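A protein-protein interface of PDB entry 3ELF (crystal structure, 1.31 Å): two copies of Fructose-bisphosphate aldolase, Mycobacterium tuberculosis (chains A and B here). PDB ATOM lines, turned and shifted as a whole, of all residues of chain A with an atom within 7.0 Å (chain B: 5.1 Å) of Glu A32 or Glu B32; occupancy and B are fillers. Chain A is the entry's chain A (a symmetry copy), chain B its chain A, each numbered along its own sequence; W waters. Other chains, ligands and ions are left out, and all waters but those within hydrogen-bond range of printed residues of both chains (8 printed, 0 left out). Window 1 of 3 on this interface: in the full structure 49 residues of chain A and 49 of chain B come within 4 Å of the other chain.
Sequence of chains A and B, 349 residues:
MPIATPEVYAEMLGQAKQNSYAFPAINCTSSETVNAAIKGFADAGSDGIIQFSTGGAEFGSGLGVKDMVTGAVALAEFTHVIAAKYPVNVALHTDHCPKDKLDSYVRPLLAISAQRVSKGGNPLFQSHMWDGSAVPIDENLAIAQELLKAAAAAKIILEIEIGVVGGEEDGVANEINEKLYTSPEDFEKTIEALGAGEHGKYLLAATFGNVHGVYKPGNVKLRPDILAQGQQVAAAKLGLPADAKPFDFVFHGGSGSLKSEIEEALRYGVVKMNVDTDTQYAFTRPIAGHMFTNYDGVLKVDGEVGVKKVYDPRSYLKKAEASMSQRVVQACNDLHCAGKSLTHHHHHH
The side-chain hydroxyl (OG) of Ser B31 sits at hydrogen-bond distance from the backbone NH (N) of Ser A31 (3.0 Å). OE1 of Glu B32 sits close to OE1 of Glu A32 (2.5 Å). The side-chain amide nitrogen (ND2) of Asn B35 is in hydrogen-bond range of the backbone carbonyl oxygen (O) of Gly A60, 2.9 Å away. The backbone NH (N) of Gly A62 sits close to the side-chain amide nitrogen (ND2) of Asn B35.
OG of Ser B30 sits close to N of Glu B32 (3.4 Å). The side-chain hydroxyl (OG1) of Thr B33 lies within hydrogen-bond range of the side-chain hydroxyl (OG) of Ser B30 (2.8 Å). The side-chain hydroxyl of Ser B31 lies within hydrogen-bond range of the side-chain carboxylate of Glu B32. O of Ser B31 lies within hydrogen-bond range of ND2 of Asn B35. OG of Ser A30 sits close to N of Glu A32 (3.4 Å). O of Ser A31 sits at hydrogen-bond distance from ND2 of Asn A35, at 3.3 Å.
Among the printed residues, merely in contact across the chains: Glu A32 with Ser B30, Ser A30 with Glu B32, Ser A30 with Ser B31, Ser A31 with Ser B30, Pro A313 with Phe B283, Leu A317 with Phe B59, Phe A59 with Leu B317, Lys A318 with Phe B59, Gly A62 with Glu B321, Glu A32 with Phe B59 and Phe A59 with Glu B32.
Of chain B, only Ser B30, Glu B32 and Phe B59 come within 4 Å of Glu A32. Of chain A, only Ser A30, Glu A32 and Phe A59 come within 4 Å of Glu B32. Of the printed residues of chain A, Ser B30 touches Ser A31 and Glu A32. Of the printed residues of chain B, Leu A317 touches Phe B59. Of the printed residues of chain B, Ser A31 touches Ser B30 and Ser B31. Val A34 touches none of the printed residues of chain B. Thr A33 touches none of the printed residues of chain B. The nearest residue of chain B that does not touch Glu A32 is Ser B31 (4.2 Å). The nearest printed residue of chain B that does not touch Leu A317 is Phe B283 (4.6 Å).
Of the 12 printed residues of chain B, 8 touch a printed residue of chain A. Along chain B the printed residues that touch a printed residue of chain A span positions 30 to 321. Of the 23 printed residues of chain A, 9 touch a printed residue of chain B. Hydrophobic or aromatic side chains of chain A within 4 Å of the printed part of chain B: Phe A59, Pro A313 and Leu A317. Among the printed residues, no Asp or Glu carboxylate lies within 4 Å of a Lys or Arg side-chain nitrogen of the other chain.
Ser A30 touches Ser B31, and with the chains exchanged Ser A31 touches Ser B30. Ser A31 touches its own counterpart, Ser B31. Glu B32 touches its own counterpart, Glu A32. Phe A59 touches Leu B317, and with the chains exchanged Leu A317 touches Phe B59. Positions printed for both chains: 30, 31, 32, 33, 34, 35, 36, 37, 59, 283, 317 and 321.
Water W5 lies within hydrogen-bond range of the side-chain hydroxyl (OG) of Ser A30 (2.6 Å), the side-chain carboxylate (OE2) of Glu B32 (2.7 Å) and the side-chain carboxylate (OE1) of Glu A32 (3.3 Å). Water W7 lies within hydrogen-bond range of the side-chain hydroxyl of Thr A29 (2.7 Å) and the side-chain carboxylate of Glu B32 (3.4 Å). Water W4 lies within hydrogen-bond range of the side-chain hydroxyl of Ser B31 (2.7 Å) and the backbone carbonyl oxygen of Thr A29 (2.9 Å). Water W2 lies within hydrogen-bond range of the side-chain carboxylate of Glu A321 and the backbone carbonyl oxygen of Phe B59. Water W1 bridges the side-chain carboxylate (OE2) of Glu B321 (2.8 Å) and the backbone carbonyl oxygen (O) of Phe A59 (2.9 Å). Water W8 bridges O of Phe B59 and ND2 of Asn A35.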
ATOM      1  N   CYS A  28      -0.568  38.101  25.880  1.00  0.00           N
ATOM      2  CA  CYS A  28      -0.432  36.664  26.111  1.00  0.00           C
ATOM      3  C   CYS A  28      -1.386  35.923  25.191  1.00  0.00           C
ATOM      4  O   CYS A  28      -2.347  36.504  24.673  1.00  0.00           O
ATOM      5  CB  CYS A  28      -0.708  36.312  27.572  1.00  0.00           C
ATOM      6  SG  CYS A  28       0.486  37.009  28.725  1.00  0.00           S
ATOM      7  N   THR A  29      -1.107  34.638  24.981  1.00  0.00           N
ATOM      8  CA  THR A  29      -1.813  33.847  23.976  1.00  0.00           C
ATOM      9  C   THR A  29      -2.099  32.427  24.459  1.00  0.00           C
ATOM     10  O   THR A  29      -2.657  31.626  23.715  1.00  0.00           O
ATOM     11  CB  THR A  29      -0.971  33.742  22.688  1.00  0.00           C
ATOM     12  OG1 THR A  29       0.334  33.254  23.021  1.00  0.00           O
ATOM     13  CG2 THR A  29      -0.842  35.101  22.006  1.00  0.00           C
ATOM     14  N   SER A  30      -1.702  32.108  25.689  1.00  0.00           N
ATOM     15  CA  SER A  30      -1.665  30.710  26.119  1.00  0.00           C
ATOM     16  C   SER A  30      -1.451  30.604  27.610  1.00  0.00           C
ATOM     17  O   SER A  30      -1.101  31.592  28.266  1.00  0.00           O
ATOM     18  CB  SER A  30      -0.496  30.004  25.442  1.00  0.00           C
ATOM     19  OG  SER A  30       0.725  30.560  25.919  1.00  0.00           O
ATOM     20  N   SER A  31      -1.616  29.394  28.144  1.00  0.00           N
ATOM     21  CA  SER A  31      -1.291  29.126  29.531  1.00  0.00           C
ATOM     22  C   SER A  31       0.177  29.440  29.844  1.00  0.00           C
ATOM     23  O   SER A  31       0.476  30.041  30.873  1.00  0.00           O
ATOM     24  CB  SER A  31      -1.644  27.678  29.880  1.00  0.00           C
ATOM     25  OG  SER A  31      -1.060  26.769  28.974  1.00  0.00           O
ATOM     26  N   GLU A  32       1.091  29.046  28.955  1.00  0.00           N
ATOM     27  CA  GLU A  32       2.514  29.270  29.220  1.00  0.00           C
ATOM     28  C   GLU A  32       2.861  30.750  29.258  1.00  0.00           C
ATOM     29  O   GLU A  32       3.649  31.175  30.104  1.00  0.00           O
ATOM     30  CB  GLU A  32       3.391  28.590  28.170  1.00  0.00           C
ATOM     31  CG  GLU A  32       3.285  27.076  28.138  1.00  0.00           C
ATOM     32  CD  GLU A  32       2.338  26.558  27.087  1.00  0.00           C
ATOM     33  OE1 GLU A  32       1.353  27.251  26.737  1.00  0.00           O
ATOM     34  OE2 GLU A  32       2.602  25.435  26.607  1.00  0.00           O
ATOM     35  N   THR A  33       2.305  31.526  28.332  1.00  0.00           N
ATOM     36  CA  THR A  33       2.628  32.951  28.278  1.00  0.00           C
ATOM     37  C   THR A  33       1.989  33.719  29.444  1.00  0.00           C
ATOM     38  O   THR A  33       2.619  34.600  30.023  1.00  0.00           O
ATOM     39  CB  THR A  33       2.318  33.581  26.907  1.00  0.00           C
ATOM     40  OG1 THR A  33       0.962  33.319  26.549  1.00  0.00           O
ATOM     41  CG2 THR A  33       3.265  33.017  25.841  1.00  0.00           C
ATOM     42  N   VAL A  34       0.762  33.359  29.821  1.00  0.00           N
ATOM     43  CA  VAL A  34       0.148  33.912  31.035  1.00  0.00           C
ATOM     44  C   VAL A  34       1.020  33.606  32.255  1.00  0.00           C
ATOM     45  O   VAL A  34       1.338  34.499  33.048  1.00  0.00           O
ATOM     46  CB  VAL A  34      -1.297  33.386  31.240  1.00  0.00           C
ATOM     47  CG1 VAL A  34      -1.794  33.691  32.649  1.00  0.00           C
ATOM     48  CG2 VAL A  34      -2.241  33.975  30.192  1.00  0.00           C
ATOM     49  N   ASN A  35       1.429  32.345  32.401  1.00  0.00           N
ATOM     50  CA  ASN A  35       2.260  31.958  33.531  1.00  0.00           C
ATOM     51  C   ASN A  35       3.573  32.742  33.551  1.00  0.00           C
ATOM     52  O   ASN A  35       4.023  33.180  34.616  1.00  0.00           O
ATOM     53  CB  ASN A  35       2.531  30.451  33.510  1.00  0.00           C
ATOM     54  CG  ASN A  35       1.370  29.643  34.054  1.00  0.00           C
ATOM     55  OD1 ASN A  35       0.573  30.143  34.849  1.00  0.00           O
ATOM     56  ND2 ASN A  35       1.277  28.390  33.635  1.00  0.00           N
ATOM     57  N   ALA A  36       4.177  32.917  32.373  1.00  0.00           N
ATOM     58  CA  ALA A  36       5.436  33.662  32.269  1.00  0.00           C
ATOM     59  C   ALA A  36       5.254  35.118  32.689  1.00  0.00           C
ATOM     60  O   ALA A  36       6.086  35.677  33.408  1.00  0.00           O
ATOM     61  CB  ALA A  36       5.989  33.584  30.855  1.00  0.00           C
ATOM     62  N   ALA A  37       4.174  35.739  32.231  1.00  0.00           N
ATOM     63  CA  ALA A  37       3.926  37.139  32.551  1.00  0.00           C
ATOM     64  C   ALA A  37       3.707  37.339  34.045  1.00  0.00           C
ATOM     65  O   ALA A  37       4.311  38.224  34.649  1.00  0.00           O
ATOM     66  CB  ALA A  37       2.763  37.670  31.749  1.00  0.00           C
ATOM     67  N   PHE A  59      -6.493  32.522  18.727  1.00  0.00           N
ATOM     68  CA  PHE A  59      -5.491  31.473  18.890  1.00  0.00           C
ATOM     69  C   PHE A  59      -5.755  30.649  20.156  1.00  0.00           C
ATOM     70  O   PHE A  59      -5.666  29.420  20.137  1.00  0.00           O
ATOM     71  CB  PHE A  59      -4.086  32.087  18.924  1.00  0.00           C
ATOM     72  CG  PHE A  59      -3.012  31.105  19.286  1.00  0.00           C
ATOM     73  CD1 PHE A  59      -2.446  30.272  18.327  1.00  0.00           C
ATOM     74  CD2 PHE A  59      -2.576  31.000  20.596  1.00  0.00           C
ATOM     75  CE1 PHE A  59      -1.457  29.359  18.678  1.00  0.00           C
ATOM     76  CE2 PHE A  59      -1.590  30.086  20.953  1.00  0.00           C
ATOM     77  CZ  PHE A  59      -1.031  29.270  19.991  1.00  0.00           C
ATOM     78  N   GLY A  60      -6.061  31.331  21.254  1.00  0.00           N
ATOM     79  CA  GLY A  60      -6.362  30.666  22.513  1.00  0.00           C
ATOM     80  C   GLY A  60      -7.566  29.744  22.454  1.00  0.00           C
ATOM     81  O   GLY A  60      -7.651  28.790  23.228  1.00  0.00           O
ATOM     82  N   GLY A  62      -8.245  27.814  19.944  1.00  0.00           N
ATOM     83  CA  GLY A  62      -7.855  26.658  19.135  1.00  0.00           C
ATOM     84  C   GLY A  62      -8.307  26.733  17.687  1.00  0.00           C
ATOM     85  O   GLY A  62      -9.289  27.408  17.344  1.00  0.00           O
ATOM     86  N   LEU A  75      -8.988  31.664  28.481  1.00  0.00           N
ATOM     87  CA  LEU A  75      -7.722  32.141  29.024  1.00  0.00           C
ATOM     88  C   LEU A  75      -7.924  32.972  30.283  1.00  0.00           C
ATOM     89  O   LEU A  75      -7.114  32.892  31.202  1.00  0.00           O
ATOM     90  CB  LEU A  75      -6.923  32.921  27.974  1.00  0.00           C
ATOM     91  CG  LEU A  75      -6.346  32.094  26.818  1.00  0.00           C
ATOM     92  CD1 LEU A  75      -5.784  33.040  25.770  1.00  0.00           C
ATOM     93  CD2 LEU A  75      -5.282  31.121  27.314  1.00  0.00           C
ATOM     94  N   PHE A  78      -8.566  30.477  33.169  1.00  0.00           N
ATOM     95  CA  PHE A  78      -7.268  29.940  33.531  1.00  0.00           C
ATOM     96  C   PHE A  78      -6.517  30.937  34.422  1.00  0.00           C
ATOM     97  O   PHE A  78      -6.009  30.578  35.485  1.00  0.00           O
ATOM     98  CB  PHE A  78      -6.462  29.625  32.262  1.00  0.00           C
ATOM     99  CG  PHE A  78      -5.041  29.221  32.532  1.00  0.00           C
ATOM    100  CD1 PHE A  78      -4.720  27.891  32.773  1.00  0.00           C
ATOM    101  CD2 PHE A  78      -4.025  30.174  32.538  1.00  0.00           C
ATOM    102  CE1 PHE A  78      -3.402  27.519  33.053  1.00  0.00           C
ATOM    103  CE2 PHE A  78      -2.719  29.805  32.807  1.00  0.00           C
ATOM    104  CZ  PHE A  78      -2.409  28.478  33.063  1.00  0.00           C
ATOM    105  N   PHE A 283      10.364  34.624  24.650  1.00  0.00           N
ATOM    106  CA  PHE A 283       9.748  33.300  24.756  1.00  0.00           C
ATOM    107  C   PHE A 283      10.365  32.325  23.748  1.00  0.00           C
ATOM    108  O   PHE A 283      10.751  31.204  24.094  1.00  0.00           O
ATOM    109  CB  PHE A 283       8.240  33.427  24.518  1.00  0.00           C
ATOM    110  CG  PHE A 283       7.449  32.182  24.863  1.00  0.00           C
ATOM    111  CD1 PHE A 283       7.023  31.958  26.169  1.00  0.00           C
ATOM    112  CD2 PHE A 283       7.132  31.245  23.878  1.00  0.00           C
ATOM    113  CE1 PHE A 283       6.282  30.822  26.494  1.00  0.00           C
ATOM    114  CE2 PHE A 283       6.392  30.104  24.194  1.00  0.00           C
ATOM    115  CZ  PHE A 283       5.972  29.896  25.498  1.00  0.00           C
ATOM    116  N   PRO A 313       7.264  18.629  25.210  1.00  0.00           N
ATOM    117  CA  PRO A 313       7.147  20.095  25.089  1.00  0.00           C
ATOM    118  C   PRO A 313       7.544  20.871  26.342  1.00  0.00           C
ATOM    119  O   PRO A 313       8.054  21.987  26.229  1.00  0.00           O
ATOM    120  CB  PRO A 313       5.671  20.304  24.727  1.00  0.00           C
ATOM    121  CG  PRO A 313       5.305  19.033  23.993  1.00  0.00           C
ATOM    122  CD  PRO A 313       6.024  17.954  24.784  1.00  0.00           C
ATOM    123  N   LEU A 317       9.492  24.442  26.799  1.00  0.00           N
ATOM    124  CA  LEU A 317       8.548  25.465  27.228  1.00  0.00           C
ATOM    125  C   LEU A 317       8.831  26.033  28.626  1.00  0.00           C
ATOM    126  O   LEU A 317       8.514  27.187  28.878  1.00  0.00           O
ATOM    127  CB  LEU A 317       7.102  24.994  27.056  1.00  0.00           C
ATOM    128  CG  LEU A 317       6.664  24.821  25.588  1.00  0.00           C
ATOM    129  CD1 LEU A 317       5.352  24.055  25.496  1.00  0.00           C
ATOM    130  CD2 LEU A 317       6.546  26.148  24.850  1.00  0.00           C
ATOM    131  N   LYS A 318       9.427  25.242  29.516  1.00  0.00           N
ATOM    132  CA  LYS A 318       9.890  25.778  30.797  1.00  0.00           C
ATOM    133  C   LYS A 318      10.932  26.873  30.562  1.00  0.00           C
ATOM    134  O   LYS A 318      10.890  27.928  31.204  1.00  0.00           O
ATOM    135  CB  LYS A 318      10.500  24.685  31.671  1.00  0.00           C
ATOM    136  CG  LYS A 318       9.504  23.734  32.308  1.00  0.00           C
ATOM    137  CD  LYS A 318      10.239  22.701  33.145  1.00  0.00           C
ATOM    138  CE  LYS A 318       9.282  21.707  33.776  1.00  0.00           C
ATOM    139  NZ  LYS A 318       9.997  20.770  34.679  1.00  0.00           N
ATOM    140  N   ALA A 320      11.343  28.650  27.790  1.00  0.00           N
ATOM    141  CA  ALA A 320      10.603  29.759  27.180  1.00  0.00           C
ATOM    142  C   ALA A 320       9.926  30.628  28.227  1.00  0.00           C
ATOM    143  O   ALA A 320      10.037  31.867  28.207  1.00  0.00           O
ATOM    144  CB  ALA A 320       9.573  29.219  26.203  1.00  0.00           C
ATOM    145  N   GLU A 321       9.205  29.973  29.133  1.00  0.00           N
ATOM    146  CA  GLU A 321       8.535  30.652  30.232  1.00  0.00           C
ATOM    147  C   GLU A 321       9.510  31.507  31.041  1.00  0.00           C
ATOM    148  O   GLU A 321       9.276  32.700  31.241  1.00  0.00           O
ATOM    149  CB  GLU A 321       7.842  29.637  31.147  1.00  0.00           C
ATOM    150  CG  GLU A 321       6.813  30.264  32.073  1.00  0.00           C
ATOM    151  CD  GLU A 321       6.405  29.376  33.233  1.00  0.00           C
ATOM    152  OE1 GLU A 321       6.510  29.833  34.390  1.00  0.00           O
ATOM    153  OE2 GLU A 321       5.967  28.234  32.998  1.00  0.00           O
ATOM    154  N   MET A 324      10.815  34.549  29.068  1.00  0.00           N
ATOM    155  CA  MET A 324       9.807  35.587  28.975  1.00  0.00           C
ATOM    156  C   MET A 324       9.599  36.297  30.317  1.00  0.00           C
ATOM    157  O   MET A 324       9.468  37.521  30.350  1.00  0.00           O
ATOM    158  CB  MET A 324       8.501  35.030  28.398  1.00  0.00           C
ATOM    159  CG  MET A 324       7.391  36.051  28.333  1.00  0.00           C
ATOM    160  SD  MET A 324       5.971  35.414  27.448  1.00  0.00           S
ATOM    161  CE  MET A 324       4.714  36.595  27.938  1.00  0.00           C
ATOM    162  N   SER A 325       9.611  35.554  31.420  1.00  0.00           N
ATOM    163  CA  SER A 325       9.476  36.181  32.738  1.00  0.00           C
ATOM    164  C   SER A 325      10.590  37.196  32.984  1.00  0.00           C
ATOM    165  O   SER A 325      10.338  38.272  33.531  1.00  0.00           O
ATOM    166  CB  SER A 325       9.468  35.135  33.850  1.00  0.00           C
ATOM    167  OG  SER A 325       8.321  34.306  33.766  1.00  0.00           O
ATOM    168  N   SER B  30      -1.109  22.082  28.707  1.00  0.00           N
ATOM    169  CA  SER B  30      -1.216  23.489  28.324  1.00  0.00           C
ATOM    170  C   SER B  30      -2.482  23.747  27.542  1.00  0.00           C
ATOM    171  O   SER B  30      -3.150  22.804  27.100  1.00  0.00           O
ATOM    172  CB  SER B  30      -0.044  23.859  27.422  1.00  0.00           C
ATOM    173  OG  SER B  30      -0.154  23.144  26.197  1.00  0.00           O
ATOM    174  N   SER B  31      -2.793  25.025  27.329  1.00  0.00           N
ATOM    175  CA  SER B  31      -3.893  25.405  26.465  1.00  0.00           C
ATOM    176  C   SER B  31      -3.718  24.854  25.044  1.00  0.00           C
ATOM    177  O   SER B  31      -4.670  24.348  24.455  1.00  0.00           O
ATOM    178  CB  SER B  31      -4.056  26.926  26.463  1.00  0.00           C
ATOM    179  OG  SER B  31      -2.843  27.577  26.158  1.00  0.00           O
ATOM    180  N   GLU B  32      -2.504  24.942  24.498  1.00  0.00           N
ATOM    181  CA  GLU B  32      -2.284  24.482  23.125  1.00  0.00           C
ATOM    182  C   GLU B  32      -2.483  22.982  22.987  1.00  0.00           C
ATOM    183  O   GLU B  32      -3.059  22.525  21.999  1.00  0.00           O
ATOM    184  CB  GLU B  32      -0.880  24.835  22.637  1.00  0.00           C
ATOM    185  CG  GLU B  32      -0.593  26.322  22.547  1.00  0.00           C
ATOM    186  CD  GLU B  32       0.131  26.873  23.748  1.00  0.00           C
ATOM    187  OE1 GLU B  32      -0.033  26.345  24.873  1.00  0.00           O
ATOM    188  OE2 GLU B  32       0.884  27.849  23.544  1.00  0.00           O
ATOM    189  N   THR B  33      -1.986  22.214  23.953  1.00  0.00           N
ATOM    190  CA  THR B  33      -2.100  20.758  23.866  1.00  0.00           C
ATOM    191  C   THR B  33      -3.542  20.290  24.103  1.00  0.00           C
ATOM    192  O   THR B  33      -4.019  19.387  23.421  1.00  0.00           O
ATOM    193  CB  THR B  33      -1.079  20.026  24.758  1.00  0.00           C
ATOM    194  OG1 THR B  33      -1.183  20.498  26.100  1.00  0.00           O
ATOM    195  CG2 THR B  33       0.342  20.250  24.227  1.00  0.00           C
ATOM    196  N   VAL B  34      -4.253  20.928  25.033  1.00  0.00           N
ATOM    197  CA  VAL B  34      -5.689  20.670  25.201  1.00  0.00           C
ATOM    198  C   VAL B  34      -6.434  20.957  23.896  1.00  0.00           C
ATOM    199  O   VAL B  34      -7.220  20.132  23.418  1.00  0.00           O
ATOM    200  CB  VAL B  34      -6.288  21.490  26.374  1.00  0.00           C
ATOM    201  CG1 VAL B  34      -7.811  21.475  26.328  1.00  0.00           C
ATOM    202  CG2 VAL B  34      -5.780  20.964  27.717  1.00  0.00           C
ATOM    203  N   ASN B  35      -6.177  22.123  23.300  1.00  0.00           N
ATOM    204  CA  ASN B  35      -6.838  22.485  22.056  1.00  0.00           C
ATOM    205  C   ASN B  35      -6.542  21.470  20.952  1.00  0.00           C
ATOM    206  O   ASN B  35      -7.442  21.097  20.189  1.00  0.00           O
ATOM    207  CB  ASN B  35      -6.429  23.894  21.619  1.00  0.00           C
ATOM    208  CG  ASN B  35      -7.182  24.977  22.365  1.00  0.00           C
ATOM    209  OD1 ASN B  35      -8.290  24.752  22.854  1.00  0.00           O
ATOM    210  ND2 ASN B  35      -6.588  26.159  22.446  1.00  0.00           N
ATOM    211  N   ALA B  36      -5.286  21.027  20.874  1.00  0.00           N
ATOM    212  CA  ALA B  36      -4.888  20.045  19.861  1.00  0.00           C
ATOM    213  C   ALA B  36      -5.620  18.720  20.058  1.00  0.00           C
ATOM    214  O   ALA B  36      -6.090  18.109  19.095  1.00  0.00           O
ATOM    215  CB  ALA B  36      -3.383  19.827  19.888  1.00  0.00           C
ATOM    216  N   ALA B  37      -5.706  18.266  21.302  1.00  0.00           N
ATOM    217  CA  ALA B  37      -6.360  16.996  21.590  1.00  0.00           C
ATOM    218  C   ALA B  37      -7.842  17.041  21.243  1.00  0.00           C
ATOM    219  O   ALA B  37      -8.352  16.142  20.576  1.00  0.00           O
ATOM    220  CB  ALA B  37      -6.144  16.602  23.031  1.00  0.00           C
ATOM    221  N   PHE B  59       3.471  21.698  35.811  1.00  0.00           N
ATOM    222  CA  PHE B  59       3.882  22.543  34.695  1.00  0.00           C
ATOM    223  C   PHE B  59       2.792  23.563  34.342  1.00  0.00           C
ATOM    224  O   PHE B  59       3.081  24.737  34.107  1.00  0.00           O
ATOM    225  CB  PHE B  59       4.231  21.678  33.478  1.00  0.00           C
ATOM    226  CG  PHE B  59       4.473  22.470  32.228  1.00  0.00           C
ATOM    227  CD1 PHE B  59       5.714  23.044  31.970  1.00  0.00           C
ATOM    228  CD2 PHE B  59       3.452  22.660  31.314  1.00  0.00           C
ATOM    229  CE1 PHE B  59       5.922  23.785  30.811  1.00  0.00           C
ATOM    230  CE2 PHE B  59       3.654  23.403  30.155  1.00  0.00           C
ATOM    231  CZ  PHE B  59       4.891  23.961  29.906  1.00  0.00           C
ATOM    232  N   PHE B 283       3.642  17.149  18.407  1.00  0.00           N
ATOM    233  CA  PHE B 283       3.584  18.569  18.754  1.00  0.00           C
ATOM    234  C   PHE B 283       4.915  19.264  18.450  1.00  0.00           C
ATOM    235  O   PHE B 283       4.955  20.324  17.816  1.00  0.00           O
ATOM    236  CB  PHE B 283       3.240  18.708  20.241  1.00  0.00           C
ATOM    237  CG  PHE B 283       2.886  20.117  20.668  1.00  0.00           C
ATOM    238  CD1 PHE B 283       1.585  20.590  20.527  1.00  0.00           C
ATOM    239  CD2 PHE B 283       3.857  20.961  21.213  1.00  0.00           C
ATOM    240  CE1 PHE B 283       1.246  21.881  20.931  1.00  0.00           C
ATOM    241  CE2 PHE B 283       3.527  22.256  21.619  1.00  0.00           C
ATOM    242  CZ  PHE B 283       2.226  22.711  21.475  1.00  0.00           C
ATOM    243  N   LEU B 317       3.352  27.498  17.041  1.00  0.00           N
ATOM    244  CA  LEU B 317       2.424  26.743  17.873  1.00  0.00           C
ATOM    245  C   LEU B 317       1.137  26.320  17.153  1.00  0.00           C
ATOM    246  O   LEU B 317       0.568  25.293  17.498  1.00  0.00           O
ATOM    247  CB  LEU B 317       2.160  27.460  19.200  1.00  0.00           C
ATOM    248  CG  LEU B 317       3.379  27.521  20.141  1.00  0.00           C
ATOM    249  CD1 LEU B 317       3.146  28.509  21.275  1.00  0.00           C
ATOM    250  CD2 LEU B 317       3.753  26.157  20.706  1.00  0.00           C
ATOM    251  N   GLU B 321       0.039  22.484  17.135  1.00  0.00           N
ATOM    252  CA  GLU B 321      -1.336  22.099  17.415  1.00  0.00           C
ATOM    253  C   GLU B 321      -1.896  21.184  16.326  1.00  0.00           C
ATOM    254  O   GLU B 321      -2.395  20.096  16.620  1.00  0.00           O
ATOM    255  CB  GLU B 321      -2.221  23.341  17.563  1.00  0.00           C
ATOM    256  CG  GLU B 321      -3.556  23.053  18.232  1.00  0.00           C
ATOM    257  CD  GLU B 321      -4.589  24.148  18.043  1.00  0.00           C
ATOM    258  OE1 GLU B 321      -5.698  23.836  17.563  1.00  0.00           O
ATOM    259  OE2 GLU B 321      -4.308  25.313  18.383  1.00  0.00           O
HETATM  260  O   HOH W   1      -4.882  27.962  17.743  1.00  0.00           O
HETATM  261  O   HOH W   2       5.832  25.687  34.117  1.00  0.00           O
HETATM  262  O   HOH W   3       1.952  23.658  24.712  1.00  0.00           O
HETATM  263  O   HOH W   4      -3.195  28.773  23.790  1.00  0.00           O
HETATM  264  O   HOH W   5       2.731  29.454  24.631  1.00  0.00           O
HETATM  265  O   HOH W   6      -4.122  27.485  21.516  1.00  0.00           O
HETATM  266  O   HOH W   7       1.599  31.004  22.409  1.00  0.00           O
HETATM  267  O   HOH W   8       2.745  26.498  31.912  1.00  0.00           O
